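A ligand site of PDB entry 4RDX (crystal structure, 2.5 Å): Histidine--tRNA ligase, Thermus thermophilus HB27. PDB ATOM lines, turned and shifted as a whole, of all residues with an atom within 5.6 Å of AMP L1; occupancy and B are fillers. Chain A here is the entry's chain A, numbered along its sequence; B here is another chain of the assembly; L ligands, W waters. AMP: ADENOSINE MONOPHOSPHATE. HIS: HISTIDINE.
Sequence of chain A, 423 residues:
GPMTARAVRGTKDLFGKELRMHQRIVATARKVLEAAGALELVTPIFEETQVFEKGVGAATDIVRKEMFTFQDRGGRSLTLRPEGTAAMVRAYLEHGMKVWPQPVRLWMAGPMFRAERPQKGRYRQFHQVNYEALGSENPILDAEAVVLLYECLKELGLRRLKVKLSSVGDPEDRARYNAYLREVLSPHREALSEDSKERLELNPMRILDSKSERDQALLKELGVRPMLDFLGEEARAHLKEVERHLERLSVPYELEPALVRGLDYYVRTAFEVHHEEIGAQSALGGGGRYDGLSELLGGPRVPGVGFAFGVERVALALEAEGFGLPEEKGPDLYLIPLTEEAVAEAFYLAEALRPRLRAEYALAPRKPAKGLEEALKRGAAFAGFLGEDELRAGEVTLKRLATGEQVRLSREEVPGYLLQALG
O of Leu 284 sits at hydrogen-bond distance from O2' of AMP L1, 2.5 Å away. O1P of AMP L1 lies within salt-bridge range of NH2 of Arg 114 (2.7 Å). The backbone carbonyl oxygen of Ala 283 sits at hydrogen-bond distance from an oxygen (O3') of AMP L1. N of Tyr 123 lies within hydrogen-bond range of N1 of AMP L1. N6 of AMP L1 lies within hydrogen-bond range of O of Tyr 123, 2.9 Å away. An oxygen (O2') of AMP L1 is in hydrogen-bond range of the backbone NH (N) of Gly 310, 3.1 Å away. An oxygen (O4') of AMP L1 is in hydrogen-bond range of the side-chain amide nitrogen (NE2) of Gln 128 (3.2 Å). O3' of AMP L1 lies within hydrogen-bond range of N of Gly 285 (3.3 Å). A nitrogen (N) of HIS L2 sits at hydrogen-bond distance from O3' of A 78 of chain B, 2.6 Å away.
An oxygen (O1P) of AMP L1 sits at hydrogen-bond distance from a nitrogen (N) of HIS L2 (3.1 Å).
The backbone carbonyl oxygen (O) of Leu 284 sits at hydrogen-bond distance from the backbone NH (N) of Gly 310, 3.0 Å away. N of Arg 114 sits at hydrogen-bond distance from O of Arg 124, 3.0 Å away. The backbone carbonyl oxygen of Pro 82 is in hydrogen-bond range of the guanidinium group of Arg 114, 2.9 Å away. The backbone carbonyl oxygen (O) of Ala 283 sits at hydrogen-bond distance from the guanidinium group (NH1) of Arg 313, 2.8 Å away. The backbone carbonyl oxygen (O) of Gly 121 lies within hydrogen-bond range of the guanidinium group (NE) of Arg 313 (2.6 Å). N of Ala 308 is in hydrogen-bond range of O of Gly 286.
An oxygen (O3P) of AMP L1 lies close to O3' of A 78 of chain B, at 3.5 Å. O of Gly 121 touches C2 of AMP L1 (3.2 Å). CA of Arg 122 touches N1 of AMP L1 (3.4 Å). Phe 126 touches AMP L1 (CD1 to C6, 3.4 Å). Ala 308 touches AMP L1. C of Phe 309 touches O4' of AMP L1, 3.9 Å away. Arg 313 touches AMP L1 (CD to O2', 3.4 Å). C 77 of chain B touches AMP L1 (O2' to O2P, 3.7 Å). Hydrophobic or aromatic side chains that line AMP L1: Tyr 123, Phe 126 and Ala 283. Of the 20 residues printed, 15 come within 4 Å of AMP L1.
Water W1 lies within hydrogen-bond range of N3 of AMP L1 (2.7 Å), OE1 of Glu 312 (2.9 Å) and N of Arg 313 (3.4 Å). Water W2 lies within hydrogen-bond range of a nitrogen (N6) of AMP L1 (3.0 Å) and the guanidinium group (NE) of Arg 122 (3.1 Å).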
ATOM      1  N   PRO A  82     -15.524   1.293  29.346  1.00  0.00           N
ATOM      2  CA  PRO A  82     -14.657   1.016  28.187  1.00  0.00           C
ATOM      3  C   PRO A  82     -14.341   2.281  27.381  1.00  0.00           C
ATOM      4  O   PRO A  82     -13.335   2.313  26.657  1.00  0.00           O
ATOM      5  CB  PRO A  82     -15.499   0.060  27.361  1.00  0.00           C
ATOM      6  CG  PRO A  82     -16.896   0.522  27.595  1.00  0.00           C
ATOM      7  CD  PRO A  82     -16.941   1.051  29.027  1.00  0.00           C
ATOM      8  N   GLU A  83     -15.172   3.310  27.513  1.00  0.00           N
ATOM      9  CA  GLU A  83     -14.974   4.569  26.799  1.00  0.00           C
ATOM     10  C   GLU A  83     -15.457   5.761  27.635  1.00  0.00           C
ATOM     11  O   GLU A  83     -16.211   5.596  28.592  1.00  0.00           O
ATOM     12  CB  GLU A  83     -15.699   4.560  25.455  1.00  0.00           C
ATOM     13  CG  GLU A  83     -17.177   4.187  25.543  1.00  0.00           C
ATOM     14  CD  GLU A  83     -18.081   5.228  24.921  1.00  0.00           C
ATOM     15  OE1 GLU A  83     -19.188   4.875  24.472  1.00  0.00           O
ATOM     16  OE2 GLU A  83     -17.683   6.414  24.888  1.00  0.00           O
ATOM     17  N   ARG A 114     -10.809  -2.521  28.578  1.00  0.00           N
ATOM     18  CA  ARG A 114     -11.273  -3.316  27.440  1.00  0.00           C
ATOM     19  C   ARG A 114     -10.701  -4.732  27.490  1.00  0.00           C
ATOM     20  O   ARG A 114      -9.708  -4.981  28.158  1.00  0.00           O
ATOM     21  CB  ARG A 114     -10.913  -2.608  26.116  1.00  0.00           C
ATOM     22  CG  ARG A 114     -11.706  -1.333  25.897  1.00  0.00           C
ATOM     23  CD  ARG A 114     -11.223  -0.515  24.713  1.00  0.00           C
ATOM     24  NE  ARG A 114     -11.896   0.784  24.695  1.00  0.00           N
ATOM     25  CZ  ARG A 114     -11.794   1.669  23.706  1.00  0.00           C
ATOM     26  NH1 ARG A 114     -11.033   1.413  22.649  1.00  0.00           N
ATOM     27  NH2 ARG A 114     -12.446   2.827  23.785  1.00  0.00           N
ATOM     28  N   GLY A 121       1.272  -0.830  22.967  1.00  0.00           N
ATOM     29  CA  GLY A 121       0.363   0.299  23.050  1.00  0.00           C
ATOM     30  C   GLY A 121      -1.103  -0.066  23.210  1.00  0.00           C
ATOM     31  O   GLY A 121      -1.980   0.775  23.019  1.00  0.00           O
ATOM     32  N   ARG A 122      -1.375  -1.325  23.548  1.00  0.00           N
ATOM     33  CA  ARG A 122      -2.755  -1.789  23.703  1.00  0.00           C
ATOM     34  C   ARG A 122      -2.867  -2.679  24.938  1.00  0.00           C
ATOM     35  O   ARG A 122      -2.351  -3.798  24.965  1.00  0.00           O
ATOM     36  CB  ARG A 122      -3.226  -2.534  22.459  1.00  0.00           C
ATOM     37  CG  ARG A 122      -4.694  -2.919  22.475  1.00  0.00           C
ATOM     38  CD  ARG A 122      -5.054  -3.736  21.256  1.00  0.00           C
ATOM     39  NE  ARG A 122      -6.499  -3.743  21.021  1.00  0.00           N
ATOM     40  CZ  ARG A 122      -7.081  -4.270  19.949  1.00  0.00           C
ATOM     41  NH1 ARG A 122      -6.344  -4.828  18.989  1.00  0.00           N
ATOM     42  NH2 ARG A 122      -8.398  -4.226  19.823  1.00  0.00           N
ATOM     43  N   TYR A 123      -3.565  -2.174  25.950  1.00  0.00           N
ATOM     44  CA  TYR A 123      -3.670  -2.882  27.218  1.00  0.00           C
ATOM     45  C   TYR A 123      -5.126  -3.121  27.606  1.00  0.00           C
ATOM     46  O   TYR A 123      -6.033  -2.696  26.887  1.00  0.00           O
ATOM     47  CB  TYR A 123      -2.932  -2.089  28.311  1.00  0.00           C
ATOM     48  CG  TYR A 123      -1.616  -1.505  27.826  1.00  0.00           C
ATOM     49  CD1 TYR A 123      -0.487  -2.304  27.690  1.00  0.00           C
ATOM     50  CD2 TYR A 123      -1.502  -0.170  27.497  1.00  0.00           C
ATOM     51  CE1 TYR A 123       0.706  -1.778  27.248  1.00  0.00           C
ATOM     52  CE2 TYR A 123      -0.316   0.361  27.050  1.00  0.00           C
ATOM     53  CZ  TYR A 123       0.793  -0.452  26.930  1.00  0.00           C
ATOM     54  OH  TYR A 123       1.982   0.066  26.487  1.00  0.00           O
ATOM     55  N   ARG A 124      -5.333  -3.798  28.726  1.00  0.00           N
ATOM     56  CA  ARG A 124      -6.684  -4.110  29.193  1.00  0.00           C
ATOM     57  C   ARG A 124      -7.171  -3.060  30.183  1.00  0.00           C
ATOM     58  O   ARG A 124      -8.365  -2.795  30.275  1.00  0.00           O
ATOM     59  CB  ARG A 124      -6.751  -5.519  29.755  1.00  0.00           C
ATOM     60  CG  ARG A 124      -6.577  -6.576  28.668  1.00  0.00           C
ATOM     61  CD  ARG A 124      -6.878  -7.974  29.157  1.00  0.00           C
ATOM     62  NE  ARG A 124      -7.023  -8.901  28.045  1.00  0.00           N
ATOM     63  CZ  ARG A 124      -7.177 -10.215  28.180  1.00  0.00           C
ATOM     64  NH1 ARG A 124      -7.183 -10.743  29.402  1.00  0.00           N
ATOM     65  NH2 ARG A 124      -7.307 -10.989  27.123  1.00  0.00           N
ATOM     66  N   PHE A 126      -6.099   0.887  30.543  1.00  0.00           N
ATOM     67  CA  PHE A 126      -5.270   1.947  30.001  1.00  0.00           C
ATOM     68  C   PHE A 126      -5.806   3.291  30.461  1.00  0.00           C
ATOM     69  O   PHE A 126      -6.816   3.337  31.145  1.00  0.00           O
ATOM     70  CB  PHE A 126      -5.184   1.840  28.465  1.00  0.00           C
ATOM     71  CG  PHE A 126      -6.501   2.010  27.767  1.00  0.00           C
ATOM     72  CD1 PHE A 126      -7.382   0.940  27.651  1.00  0.00           C
ATOM     73  CD2 PHE A 126      -6.851   3.218  27.213  1.00  0.00           C
ATOM     74  CE1 PHE A 126      -8.600   1.102  27.004  1.00  0.00           C
ATOM     75  CE2 PHE A 126      -8.052   3.382  26.563  1.00  0.00           C
ATOM     76  CZ  PHE A 126      -8.932   2.322  26.456  1.00  0.00           C
ATOM     77  N   GLN A 128      -7.008   7.346  29.494  1.00  0.00           N
ATOM     78  CA  GLN A 128      -7.467   8.190  28.396  1.00  0.00           C
ATOM     79  C   GLN A 128      -7.678   9.629  28.837  1.00  0.00           C
ATOM     80  O   GLN A 128      -8.006   9.899  30.003  1.00  0.00           O
ATOM     81  CB  GLN A 128      -8.767   7.651  27.812  1.00  0.00           C
ATOM     82  CG  GLN A 128      -8.645   7.096  26.401  1.00  0.00           C
ATOM     83  CD  GLN A 128      -9.966   6.527  25.903  1.00  0.00           C
ATOM     84  OE1 GLN A 128     -11.020   6.800  26.471  1.00  0.00           O
ATOM     85  NE2 GLN A 128      -9.897   5.734  24.834  1.00  0.00           N
ATOM     86  N   ALA A 283      -2.409   4.866  16.295  1.00  0.00           N
ATOM     87  CA  ALA A 283      -3.348   5.943  16.625  1.00  0.00           C
ATOM     88  C   ALA A 283      -3.127   6.449  18.046  1.00  0.00           C
ATOM     89  O   ALA A 283      -3.414   5.741  19.019  1.00  0.00           O
ATOM     90  CB  ALA A 283      -4.779   5.473  16.427  1.00  0.00           C
ATOM     91  N   LEU A 284      -2.601   7.659  18.161  1.00  0.00           N
ATOM     92  CA  LEU A 284      -2.411   8.328  19.441  1.00  0.00           C
ATOM     93  C   LEU A 284      -3.745   8.713  20.052  1.00  0.00           C
ATOM     94  O   LEU A 284      -3.970   8.559  21.268  1.00  0.00           O
ATOM     95  CB  LEU A 284      -1.571   9.587  19.225  1.00  0.00           C
ATOM     96  CG  LEU A 284      -0.182   9.673  19.870  1.00  0.00           C
ATOM     97  CD1 LEU A 284       0.550   8.346  19.787  1.00  0.00           C
ATOM     98  CD2 LEU A 284       0.623  10.773  19.194  1.00  0.00           C
ATOM     99  N   GLY A 285      -4.631   9.208  19.203  1.00  0.00           N
ATOM    100  CA  GLY A 285      -5.942   9.645  19.621  1.00  0.00           C
ATOM    101  C   GLY A 285      -6.852   9.869  18.432  1.00  0.00           C
ATOM    102  O   GLY A 285      -6.383   9.969  17.291  1.00  0.00           O
ATOM    103  N   GLY A 286      -8.146   9.956  18.683  1.00  0.00           N
ATOM    104  CA  GLY A 286      -9.110  10.142  17.622  1.00  0.00           C
ATOM    105  C   GLY A 286     -10.438  10.600  18.175  1.00  0.00           C
ATOM    106  O   GLY A 286     -10.676  10.561  19.383  1.00  0.00           O
ATOM    107  N   ALA A 308     -10.676  11.469  22.119  1.00  0.00           N
ATOM    108  CA  ALA A 308      -9.997  10.773  23.204  1.00  0.00           C
ATOM    109  C   ALA A 308      -8.609  10.363  22.738  1.00  0.00           C
ATOM    110  O   ALA A 308      -8.432   9.998  21.575  1.00  0.00           O
ATOM    111  CB  ALA A 308     -10.792   9.560  23.636  1.00  0.00           C
ATOM    112  N   PHE A 309      -7.628  10.457  23.623  1.00  0.00           N
ATOM    113  CA  PHE A 309      -6.294   9.935  23.314  1.00  0.00           C
ATOM    114  C   PHE A 309      -5.698   9.109  24.453  1.00  0.00           C
ATOM    115  O   PHE A 309      -6.107   9.240  25.620  1.00  0.00           O
ATOM    116  CB  PHE A 309      -5.329  11.036  22.818  1.00  0.00           C
ATOM    117  CG  PHE A 309      -4.822  11.965  23.882  1.00  0.00           C
ATOM    118  CD1 PHE A 309      -3.855  11.567  24.795  1.00  0.00           C
ATOM    119  CD2 PHE A 309      -5.272  13.285  23.924  1.00  0.00           C
ATOM    120  CE1 PHE A 309      -3.374  12.440  25.755  1.00  0.00           C
ATOM    121  CE2 PHE A 309      -4.794  14.161  24.871  1.00  0.00           C
ATOM    122  CZ  PHE A 309      -3.842  13.748  25.791  1.00  0.00           C
ATOM    123  N   GLY A 310      -4.736   8.244  24.101  1.00  0.00           N
ATOM    124  CA  GLY A 310      -4.134   7.337  25.057  1.00  0.00           C
ATOM    125  C   GLY A 310      -2.842   7.844  25.643  1.00  0.00           C
ATOM    126  O   GLY A 310      -1.855   8.030  24.922  1.00  0.00           O
ATOM    127  N   GLU A 312      -0.642   6.363  27.453  1.00  0.00           N
ATOM    128  CA  GLU A 312       0.439   5.401  27.215  1.00  0.00           C
ATOM    129  C   GLU A 312       1.092   5.598  25.849  1.00  0.00           C
ATOM    130  O   GLU A 312       2.325   5.723  25.750  1.00  0.00           O
ATOM    131  CB  GLU A 312      -0.065   3.965  27.339  1.00  0.00           C
ATOM    132  CG  GLU A 312      -0.358   3.502  28.757  1.00  0.00           C
ATOM    133  CD  GLU A 312      -1.726   3.944  29.248  1.00  0.00           C
ATOM    134  OE1 GLU A 312      -2.500   4.485  28.422  1.00  0.00           O
ATOM    135  OE2 GLU A 312      -2.018   3.751  30.439  1.00  0.00           O
ATOM    136  N   ARG A 313       0.279   5.629  24.794  1.00  0.00           N
ATOM    137  CA  ARG A 313       0.803   5.764  23.434  1.00  0.00           C
ATOM    138  C   ARG A 313       1.503   7.096  23.236  1.00  0.00           C
ATOM    139  O   ARG A 313       2.476   7.198  22.491  1.00  0.00           O
ATOM    140  CB  ARG A 313      -0.317   5.593  22.407  1.00  0.00           C
ATOM    141  CG  ARG A 313      -1.042   4.261  22.514  1.00  0.00           C
ATOM    142  CD  ARG A 313      -1.895   3.968  21.281  1.00  0.00           C
ATOM    143  NE  ARG A 313      -2.553   2.665  21.380  1.00  0.00           N
ATOM    144  CZ  ARG A 313      -3.466   2.219  20.525  1.00  0.00           C
ATOM    145  NH1 ARG A 313      -3.844   2.969  19.498  1.00  0.00           N
ATOM    146  NH2 ARG A 313      -3.998   1.019  20.710  1.00  0.00           N
ATOM    147  P     C B  77     -14.792  -3.749  14.181  1.00  0.00           P
ATOM    148  OP1   C B  77     -16.232  -3.403  14.294  1.00  0.00           O
ATOM    149  OP2   C B  77     -14.173  -3.889  12.848  1.00  0.00           O
ATOM    150  O5'   C B  77     -13.983  -2.653  14.995  1.00  0.00           O
ATOM    151  C5'   C B  77     -14.586  -1.968  16.096  1.00  0.00           C
ATOM    152  C4'   C B  77     -13.542  -1.410  17.037  1.00  0.00           C
ATOM    153  O4'   C B  77     -12.454  -2.354  17.173  1.00  0.00           O
ATOM    154  C3'   C B  77     -12.866  -0.111  16.607  1.00  0.00           C
ATOM    155  O3'   C B  77     -13.644   1.036  16.888  1.00  0.00           O
ATOM    156  C2'   C B  77     -11.548  -0.158  17.369  1.00  0.00           C
ATOM    157  O2'   C B  77     -11.740   0.210  18.729  1.00  0.00           O
ATOM    158  C1'   C B  77     -11.230  -1.654  17.322  1.00  0.00           C
ATOM    159  N1    C B  77     -10.350  -1.976  16.179  1.00  0.00           N
ATOM    160  C2    C B  77      -8.973  -1.813  16.347  1.00  0.00           C
ATOM    161  O2    C B  77      -8.547  -1.416  17.438  1.00  0.00           O
ATOM    162  N3    C B  77      -8.152  -2.098  15.315  1.00  0.00           N
ATOM    163  C4    C B  77      -8.660  -2.519  14.154  1.00  0.00           C
ATOM    164  N4    C B  77      -7.802  -2.795  13.160  1.00  0.00           N
ATOM    165  C5    C B  77     -10.053  -2.693  13.957  1.00  0.00           C
ATOM    166  C6    C B  77     -10.863  -2.416  14.986  1.00  0.00           C
ATOM    167  P     A B  78     -13.793   2.205  15.805  1.00  0.00           P
ATOM    168  OP1   A B  78     -13.932   1.605  14.456  1.00  0.00           O
ATOM    169  OP2   A B  78     -12.731   3.208  16.059  1.00  0.00           O
ATOM    170  O5'   A B  78     -15.184   2.884  16.200  1.00  0.00           O
ATOM    171  C5'   A B  78     -16.017   2.291  17.186  1.00  0.00           C
ATOM    172  C4'   A B  78     -15.892   2.985  18.509  1.00  0.00           C
ATOM    173  O4'   A B  78     -16.433   2.145  19.566  1.00  0.00           O
ATOM    174  C3'   A B  78     -14.475   3.284  18.974  1.00  0.00           C
ATOM    175  O3'   A B  78     -13.932   4.457  18.380  1.00  0.00           O
ATOM    176  C2'   A B  78     -14.611   3.377  20.488  1.00  0.00           C
ATOM    177  O2'   A B  78     -15.142   4.632  20.867  1.00  0.00           O
ATOM    178  C1'   A B  78     -15.678   2.304  20.745  1.00  0.00           C
ATOM    179  N9    A B  78     -15.078   1.005  21.113  1.00  0.00           N
ATOM    180  C8    A B  78     -14.084   0.314  20.468  1.00  0.00           C
ATOM    181  N7    A B  78     -13.769  -0.825  21.024  1.00  0.00           N
ATOM    182  C5    A B  78     -14.616  -0.897  22.120  1.00  0.00           C
ATOM    183  C6    A B  78     -14.785  -1.871  23.117  1.00  0.00           C
ATOM    184  N6    A B  78     -14.068  -2.988  23.175  1.00  0.00           N
ATOM    185  N1    A B  78     -15.730  -1.643  24.067  1.00  0.00           N
ATOM    186  C2    A B  78     -16.445  -0.514  23.996  1.00  0.00           C
ATOM    187  N3    A B  78     -16.375   0.475  23.106  1.00  0.00           N
ATOM    188  C4    A B  78     -15.440   0.216  22.181  1.00  0.00           C
HETATM  189  P   AMP L   1     -10.825   4.724  20.845  1.00  0.00           P
HETATM  190  O1P AMP L   1     -11.734   4.750  22.059  1.00  0.00           O
HETATM  191  O2P AMP L   1     -10.652   3.360  20.244  1.00  0.00           O
HETATM  192  O3P AMP L   1     -11.083   5.833  19.868  1.00  0.00           O
HETATM  193  O5' AMP L   1      -9.402   5.073  21.484  1.00  0.00           O
HETATM  194  C5' AMP L   1      -8.862   6.390  21.392  1.00  0.00           C
HETATM  195  C4' AMP L   1      -7.396   6.384  21.753  1.00  0.00           C
HETATM  196  O4' AMP L   1      -7.231   5.753  23.047  1.00  0.00           O
HETATM  197  C3' AMP L   1      -6.501   5.582  20.821  1.00  0.00           C
HETATM  198  O3' AMP L   1      -6.064   6.329  19.698  1.00  0.00           O
HETATM  199  C2' AMP L   1      -5.364   5.126  21.729  1.00  0.00           C
HETATM  200  O2' AMP L   1      -4.392   6.149  21.867  1.00  0.00           O
HETATM  201  C1' AMP L   1      -6.084   4.939  23.060  1.00  0.00           C
HETATM  202  N9  AMP L   1      -6.502   3.545  23.286  1.00  0.00           N
HETATM  203  C8  AMP L   1      -7.654   2.995  22.845  1.00  0.00           C
HETATM  204  N7  AMP L   1      -7.749   1.692  23.222  1.00  0.00           N
HETATM  205  C5  AMP L   1      -6.638   1.390  23.926  1.00  0.00           C
HETATM  206  C6  AMP L   1      -6.103   0.195  24.615  1.00  0.00           C
HETATM  207  N6  AMP L   1      -6.783  -0.979  24.630  1.00  0.00           N
HETATM  208  N1  AMP L   1      -4.910   0.312  25.235  1.00  0.00           N
HETATM  209  C2  AMP L   1      -4.221   1.467  25.228  1.00  0.00           C
HETATM  210  N3  AMP L   1      -4.643   2.583  24.623  1.00  0.00           N
HETATM  211  C4  AMP L   1      -5.821   2.615  23.967  1.00  0.00           C
HETATM  212  N   HIS L   2     -13.247   6.452  19.884  1.00  0.00           N
HETATM  213  CA  HIS L   2     -14.068   7.657  19.846  1.00  0.00           C
HETATM  214  C   HIS L   2     -13.875   8.351  18.511  1.00  0.00           C
HETATM  215  O   HIS L   2     -14.737   9.112  18.061  1.00  0.00           O
HETATM  216  CB  HIS L   2     -13.690   8.586  21.005  1.00  0.00           C
HETATM  217  CG  HIS L   2     -14.523   9.835  21.078  1.00  0.00           C
HETATM  218  ND1 HIS L   2     -15.631  10.048  20.293  1.00  0.00           N
HETATM  219  CD2 HIS L   2     -14.389  10.931  21.853  1.00  0.00           C
HETATM  220  CE1 HIS L   2     -16.144  11.219  20.574  1.00  0.00           C
HETATM  221  NE2 HIS L   2     -15.418  11.785  21.527  1.00  0.00           N
HETATM  222  OXT HIS L   2     -12.853   8.166  17.852  1.00  0.00           O
HETATM  223  O   HOH W   1      -2.758   4.251  25.529  1.00  0.00           O
HETATM  224  O   HOH W   2      -8.594  -2.764  23.117  1.00  0.00           O
